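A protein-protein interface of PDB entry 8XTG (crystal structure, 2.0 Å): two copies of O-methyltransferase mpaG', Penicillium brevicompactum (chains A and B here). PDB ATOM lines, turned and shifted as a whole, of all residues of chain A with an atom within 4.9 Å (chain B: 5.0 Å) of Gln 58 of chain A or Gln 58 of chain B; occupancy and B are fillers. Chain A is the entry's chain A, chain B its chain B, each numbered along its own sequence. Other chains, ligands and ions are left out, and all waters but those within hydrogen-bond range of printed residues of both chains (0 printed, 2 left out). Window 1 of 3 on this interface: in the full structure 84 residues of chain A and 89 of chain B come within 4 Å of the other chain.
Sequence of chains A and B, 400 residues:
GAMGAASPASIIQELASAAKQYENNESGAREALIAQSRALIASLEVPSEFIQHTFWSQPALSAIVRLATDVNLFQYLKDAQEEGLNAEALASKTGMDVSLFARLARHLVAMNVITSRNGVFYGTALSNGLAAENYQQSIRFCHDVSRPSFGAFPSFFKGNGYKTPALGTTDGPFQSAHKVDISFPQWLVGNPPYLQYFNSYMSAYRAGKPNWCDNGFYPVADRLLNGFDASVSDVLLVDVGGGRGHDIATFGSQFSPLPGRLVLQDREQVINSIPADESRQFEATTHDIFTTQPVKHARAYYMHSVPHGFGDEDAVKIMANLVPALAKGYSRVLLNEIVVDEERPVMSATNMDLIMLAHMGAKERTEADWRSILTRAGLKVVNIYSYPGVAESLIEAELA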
ATOM      1  N   HIS A  53     -10.053  22.959  14.489  1.00  0.00           N
ATOM      2  CA  HIS A  53      -9.364  24.199  14.833  1.00  0.00           C
ATOM      3  C   HIS A  53      -7.854  24.062  14.674  1.00  0.00           C
ATOM      4  O   HIS A  53      -7.195  24.974  14.160  1.00  0.00           O
ATOM      5  CB  HIS A  53      -9.731  24.645  16.251  1.00  0.00           C
ATOM      6  CG  HIS A  53      -9.141  25.971  16.632  1.00  0.00           C
ATOM      7  ND1 HIS A  53      -7.816  26.127  16.982  1.00  0.00           N
ATOM      8  CD2 HIS A  53      -9.680  27.214  16.646  1.00  0.00           C
ATOM      9  CE1 HIS A  53      -7.577  27.402  17.241  1.00  0.00           C
ATOM     10  NE2 HIS A  53      -8.691  28.083  17.039  1.00  0.00           N
ATOM     11  N   THR A  54      -7.287  22.928  15.092  1.00  0.00           N
ATOM     12  CA  THR A  54      -5.841  22.757  15.017  1.00  0.00           C
ATOM     13  C   THR A  54      -5.369  22.646  13.572  1.00  0.00           C
ATOM     14  O   THR A  54      -4.391  23.294  13.177  1.00  0.00           O
ATOM     15  CB  THR A  54      -5.411  21.525  15.820  1.00  0.00           C
ATOM     16  OG1 THR A  54      -5.846  21.665  17.175  1.00  0.00           O
ATOM     17  CG2 THR A  54      -3.889  21.355  15.795  1.00  0.00           C
ATOM     18  N   TRP A  56      -7.365  22.930  10.539  1.00  0.00           N
ATOM     19  CA  TRP A  56      -8.018  23.714   9.490  1.00  0.00           C
ATOM     20  C   TRP A  56      -7.926  25.203   9.801  1.00  0.00           C
ATOM     21  O   TRP A  56      -7.282  25.941   9.053  1.00  0.00           O
ATOM     22  CB  TRP A  56      -9.484  23.315   9.295  1.00  0.00           C
ATOM     23  CG  TRP A  56      -9.813  21.854   9.171  1.00  0.00           C
ATOM     24  CD1 TRP A  56      -8.963  20.788   9.272  1.00  0.00           C
ATOM     25  CD2 TRP A  56     -11.113  21.308   8.920  1.00  0.00           C
ATOM     26  NE1 TRP A  56      -9.657  19.613   9.098  1.00  0.00           N
ATOM     27  CE2 TRP A  56     -10.979  19.906   8.880  1.00  0.00           C
ATOM     28  CE3 TRP A  56     -12.379  21.874   8.726  1.00  0.00           C
ATOM     29  CZ2 TRP A  56     -12.064  19.057   8.655  1.00  0.00           C
ATOM     30  CZ3 TRP A  56     -13.455  21.031   8.501  1.00  0.00           C
ATOM     31  CH2 TRP A  56     -13.289  19.636   8.469  1.00  0.00           C
ATOM     32  N   SER A  57      -8.565  25.666  10.880  1.00  0.00           N
ATOM     33  CA  SER A  57      -8.606  27.091  11.205  1.00  0.00           C
ATOM     34  C   SER A  57      -7.212  27.707  11.243  1.00  0.00           C
ATOM     35  O   SER A  57      -6.953  28.728  10.595  1.00  0.00           O
ATOM     36  CB  SER A  57      -9.300  27.299  12.554  1.00  0.00           C
ATOM     37  OG  SER A  57     -10.586  26.707  12.566  1.00  0.00           O
ATOM     38  N   GLN A  58      -6.307  27.103  12.005  1.00  0.00           N
ATOM     39  CA  GLN A  58      -4.997  27.691  12.246  1.00  0.00           C
ATOM     40  C   GLN A  58      -4.083  27.649  11.022  1.00  0.00           C
ATOM     41  O   GLN A  58      -3.401  28.644  10.755  1.00  0.00           O
ATOM     42  CB  GLN A  58      -4.328  27.006  13.439  1.00  0.00           C
ATOM     43  CG  GLN A  58      -4.993  27.334  14.760  1.00  0.00           C
ATOM     44  CD  GLN A  58      -4.807  28.790  15.156  1.00  0.00           C
ATOM     45  OE1 GLN A  58      -5.635  29.364  15.860  1.00  0.00           O
ATOM     46  NE2 GLN A  58      -3.712  29.392  14.703  1.00  0.00           N
ATOM     47  N   PRO A  59      -4.001  26.542  10.268  1.00  0.00           N
ATOM     48  CA  PRO A  59      -3.188  26.590   9.041  1.00  0.00           C
ATOM     49  C   PRO A  59      -3.753  27.532   7.991  1.00  0.00           C
ATOM     50  O   PRO A  59      -2.974  28.158   7.258  1.00  0.00           O
ATOM     51  CB  PRO A  59      -3.180  25.131   8.558  1.00  0.00           C
ATOM     52  CG  PRO A  59      -3.465  24.331   9.764  1.00  0.00           C
ATOM     53  CD  PRO A  59      -4.426  25.163  10.566  1.00  0.00           C
ATOM     54  N   ALA A  60      -5.081  27.659   7.902  1.00  0.00           N
ATOM     55  CA  ALA A  60      -5.673  28.631   6.986  1.00  0.00           C
ATOM     56  C   ALA A  60      -5.466  30.061   7.480  1.00  0.00           C
ATOM     57  O   ALA A  60      -5.263  30.975   6.674  1.00  0.00           O
ATOM     58  CB  ALA A  60      -7.161  28.338   6.794  1.00  0.00           C
ATOM     59  N   LEU A  61      -5.508  30.275   8.798  1.00  0.00           N
ATOM     60  CA  LEU A  61      -5.317  31.619   9.341  1.00  0.00           C
ATOM     61  C   LEU A  61      -3.907  32.132   9.068  1.00  0.00           C
ATOM     62  O   LEU A  61      -3.729  33.274   8.624  1.00  0.00           O
ATOM     63  CB  LEU A  61      -5.609  31.631  10.843  1.00  0.00           C
ATOM     64  CG  LEU A  61      -5.418  32.978  11.549  1.00  0.00           C
ATOM     65  CD1 LEU A  61      -6.406  34.013  11.015  1.00  0.00           C
ATOM     66  CD2 LEU A  61      -5.535  32.841  13.064  1.00  0.00           C
ATOM     67  N   SER A  62      -2.891  31.302   9.341  1.00  0.00           N
ATOM     68  CA  SER A  62      -1.509  31.682   9.046  1.00  0.00           C
ATOM     69  C   SER A  62      -1.320  31.994   7.569  1.00  0.00           C
ATOM     70  O   SER A  62      -0.606  32.940   7.212  1.00  0.00           O
ATOM     71  CB  SER A  62      -0.553  30.563   9.467  1.00  0.00           C
ATOM     72  OG  SER A  62      -0.367  30.564  10.866  1.00  0.00           O
ATOM     73  N   MET A 111     -12.188  34.384  12.704  1.00  0.00           N
ATOM     74  CA  MET A 111     -11.065  34.177  13.606  1.00  0.00           C
ATOM     75  C   MET A 111     -10.761  35.413  14.442  1.00  0.00           C
ATOM     76  O   MET A 111      -9.721  35.458  15.107  1.00  0.00           O
ATOM     77  CB  MET A 111      -9.818  33.763  12.821  1.00  0.00           C
ATOM     78  CG  MET A 111      -9.962  32.426  12.113  1.00  0.00           C
ATOM     79  SD  MET A 111     -10.195  31.057  13.238  1.00  0.00           S
ATOM     80  CE  MET A 111      -8.527  30.771  13.835  1.00  0.00           C
ATOM     81  N   HIS B  53       1.291  32.885  19.137  1.00  0.00           N
ATOM     82  CA  HIS B  53       0.305  31.809  19.143  1.00  0.00           C
ATOM     83  C   HIS B  53       0.014  31.314  17.732  1.00  0.00           C
ATOM     84  O   HIS B  53      -0.027  30.103  17.486  1.00  0.00           O
ATOM     85  CB  HIS B  53      -0.986  32.257  19.827  1.00  0.00           C
ATOM     86  CG  HIS B  53      -1.996  31.159  19.959  1.00  0.00           C
ATOM     87  ND1 HIS B  53      -2.035  30.310  21.044  1.00  0.00           N
ATOM     88  CD2 HIS B  53      -2.975  30.743  19.121  1.00  0.00           C
ATOM     89  CE1 HIS B  53      -3.007  29.431  20.879  1.00  0.00           C
ATOM     90  NE2 HIS B  53      -3.592  29.670  19.720  1.00  0.00           N
ATOM     91  N   THR B  54      -0.194  32.239  16.788  1.00  0.00           N
ATOM     92  CA  THR B  54      -0.533  31.840  15.423  1.00  0.00           C
ATOM     93  C   THR B  54       0.619  31.103  14.754  1.00  0.00           C
ATOM     94  O   THR B  54       0.402  30.115  14.040  1.00  0.00           O
ATOM     95  CB  THR B  54      -0.927  33.065  14.594  1.00  0.00           C
ATOM     96  OG1 THR B  54      -1.938  33.799  15.286  1.00  0.00           O
ATOM     97  CG2 THR B  54      -1.471  32.650  13.233  1.00  0.00           C
ATOM     98  N   TRP B  56       3.860  30.136  16.287  1.00  0.00           N
ATOM     99  CA  TRP B  56       4.714  29.218  17.039  1.00  0.00           C
ATOM    100  C   TRP B  56       3.905  28.092  17.672  1.00  0.00           C
ATOM    101  O   TRP B  56       4.102  26.925  17.327  1.00  0.00           O
ATOM    102  CB  TRP B  56       5.518  29.925  18.141  1.00  0.00           C
ATOM    103  CG  TRP B  56       6.309  31.136  17.742  1.00  0.00           C
ATOM    104  CD1 TRP B  56       6.522  31.616  16.480  1.00  0.00           C
ATOM    105  CD2 TRP B  56       7.090  31.953  18.620  1.00  0.00           C
ATOM    106  NE1 TRP B  56       7.329  32.731  16.533  1.00  0.00           N
ATOM    107  CE2 TRP B  56       7.703  32.948  17.833  1.00  0.00           C
ATOM    108  CE3 TRP B  56       7.321  31.947  20.002  1.00  0.00           C
ATOM    109  CZ2 TRP B  56       8.528  33.932  18.384  1.00  0.00           C
ATOM    110  CZ3 TRP B  56       8.146  32.919  20.545  1.00  0.00           C
ATOM    111  CH2 TRP B  56       8.735  33.902  19.738  1.00  0.00           C
ATOM    112  N   SER B  57       2.994  28.423  18.597  1.00  0.00           N
ATOM    113  CA  SER B  57       2.262  27.398  19.342  1.00  0.00           C
ATOM    114  C   SER B  57       1.528  26.450  18.406  1.00  0.00           C
ATOM    115  O   SER B  57       1.679  25.224  18.493  1.00  0.00           O
ATOM    116  CB  SER B  57       1.268  28.052  20.307  1.00  0.00           C
ATOM    117  OG  SER B  57       1.864  29.116  21.023  1.00  0.00           O
ATOM    118  N   GLN B  58       0.730  27.009  17.493  1.00  0.00           N
ATOM    119  CA  GLN B  58      -0.119  26.167  16.654  1.00  0.00           C
ATOM    120  C   GLN B  58       0.685  25.312  15.683  1.00  0.00           C
ATOM    121  O   GLN B  58       0.384  24.111  15.565  1.00  0.00           O
ATOM    122  CB  GLN B  58      -1.162  27.040  15.953  1.00  0.00           C
ATOM    123  CG  GLN B  58      -2.178  27.593  16.932  1.00  0.00           C
ATOM    124  CD  GLN B  58      -3.059  26.501  17.525  1.00  0.00           C
ATOM    125  OE1 GLN B  58      -3.328  25.482  16.882  1.00  0.00           O
ATOM    126  NE2 GLN B  58      -3.517  26.713  18.753  1.00  0.00           N
ATOM    127  N   PRO B  59       1.697  25.828  14.973  1.00  0.00           N
ATOM    128  CA  PRO B  59       2.519  24.919  14.155  1.00  0.00           C
ATOM    129  C   PRO B  59       3.227  23.853  14.975  1.00  0.00           C
ATOM    130  O   PRO B  59       3.259  22.681  14.573  1.00  0.00           O
ATOM    131  CB  PRO B  59       3.513  25.869  13.475  1.00  0.00           C
ATOM    132  CG  PRO B  59       2.817  27.166  13.444  1.00  0.00           C
ATOM    133  CD  PRO B  59       2.044  27.238  14.720  1.00  0.00           C
ATOM    134  N   ALA B  60       3.800  24.225  16.121  1.00  0.00           N
ATOM    135  CA  ALA B  60       4.414  23.222  16.984  1.00  0.00           C
ATOM    136  C   ALA B  60       3.379  22.244  17.528  1.00  0.00           C
ATOM    137  O   ALA B  60       3.689  21.065  17.729  1.00  0.00           O
ATOM    138  CB  ALA B  60       5.168  23.906  18.125  1.00  0.00           C
ATOM    139  N   LEU B  61       2.141  22.701  17.750  1.00  0.00           N
ATOM    140  CA  LEU B  61       1.101  21.799  18.235  1.00  0.00           C
ATOM    141  C   LEU B  61       0.691  20.796  17.163  1.00  0.00           C
ATOM    142  O   LEU B  61       0.533  19.605  17.450  1.00  0.00           O
ATOM    143  CB  LEU B  61      -0.116  22.593  18.711  1.00  0.00           C
ATOM    144  CG  LEU B  61      -1.303  21.738  19.163  1.00  0.00           C
ATOM    145  CD1 LEU B  61      -0.923  20.936  20.395  1.00  0.00           C
ATOM    146  CD2 LEU B  61      -2.527  22.598  19.435  1.00  0.00           C
ATOM    147  N   SER B  62       0.503  21.261  15.926  1.00  0.00           N
ATOM    148  CA  SER B  62       0.235  20.343  14.823  1.00  0.00           C
ATOM    149  C   SER B  62       1.334  19.297  14.706  1.00  0.00           C
ATOM    150  O   SER B  62       1.058  18.101  14.547  1.00  0.00           O
ATOM    151  CB  SER B  62       0.106  21.119  13.514  1.00  0.00           C
ATOM    152  OG  SER B  62      -1.141  21.772  13.440  1.00  0.00           O
ATOM    153  N   ALA B  63       2.592  19.736  14.792  1.00  0.00           N
ATOM    154  CA  ALA B  63       3.719  18.830  14.589  1.00  0.00           C
ATOM    155  C   ALA B  63       3.793  17.777  15.682  1.00  0.00           C
ATOM    156  O   ALA B  63       4.066  16.605  15.401  1.00  0.00           O
ATOM    157  CB  ALA B  63       5.024  19.621  14.527  1.00  0.00           C
ATOM    158  N   MET B 111      -0.544  23.508  25.921  1.00  0.00           N
ATOM    159  CA  MET B 111      -1.569  23.682  24.903  1.00  0.00           C
ATOM    160  C   MET B 111      -2.894  23.039  25.301  1.00  0.00           C
ATOM    161  O   MET B 111      -3.808  22.964  24.472  1.00  0.00           O
ATOM    162  CB  MET B 111      -1.088  23.106  23.566  1.00  0.00           C
ATOM    163  CG  MET B 111      -0.045  23.978  22.861  1.00  0.00           C
ATOM    164  SD  MET B 111      -0.469  25.716  22.651  1.00  0.00           S
ATOM    165  CE  MET B 111      -2.052  25.601  21.812  1.00  0.00           C
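O of Thr 54 of chain B lies within hydrogen-bond range of OG of Ser 62 of chain A, at 3.3 Å.
Along chain A the printed residues that touch a printed residue of chain B span positions 54 to 62.
Of the 11 printed residues of chain B, 3 touch a printed residue of chain A.
Among the printed residues, no Asp or Glu carboxylate lies within 4 Å of a Lys or Arg side-chain nitrogen of the other chain.
Gln 58 of chain A touches just one residue of chain B: Gln 58 (3.2 Å).
Of the printed residues of chain B, Ser 62 of chain A touches Thr 54.
Printed residues of chain B within 4 Å of Thr 54 of chain A: Ser 62 (3.6 Å).
Printed residues of chain A within 4 Å of Thr 54 of chain B: Ser 62.
Of the printed residues of chain A, Ser 62 of chain B touches Thr 54 (3.6 Å).
Met 111 of chain A touches none of the printed residues of chain B.
The nearest printed residue of chain B that does not touch Ser 62 of chain A is Pro 59 of chain B (5.3 Å).
The backbone carbonyl oxygen (O) of His 53 of chain A is in hydrogen-bond range of the backbone NH (N) of Gln 58 of chain A (3.2 Å).
A ring nitrogen (NE2) of His 53 of chain B is in hydrogen-bond range of the side-chain amide nitrogen of Gln 58 of chain B (3.1 Å).
Among the printed residues, pairs that only touch across the chains: Gln 58 of chain A with Gln 58 of chain B (3.2 Å) and Thr 54 of chain A with Ser 62 of chain B (3.6 Å).
Thr 54 of chain A touches Ser 62 of chain B, and with the chains exchanged Ser 62 of chain A touches Thr 54 of chain B.
Gln 58 of chain B touches its own counterpart, Gln 58 of chain A.
Of the 3 pairs that touch across the chains among the printed residues, 3 have their exchanged pair printed and touching as well.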
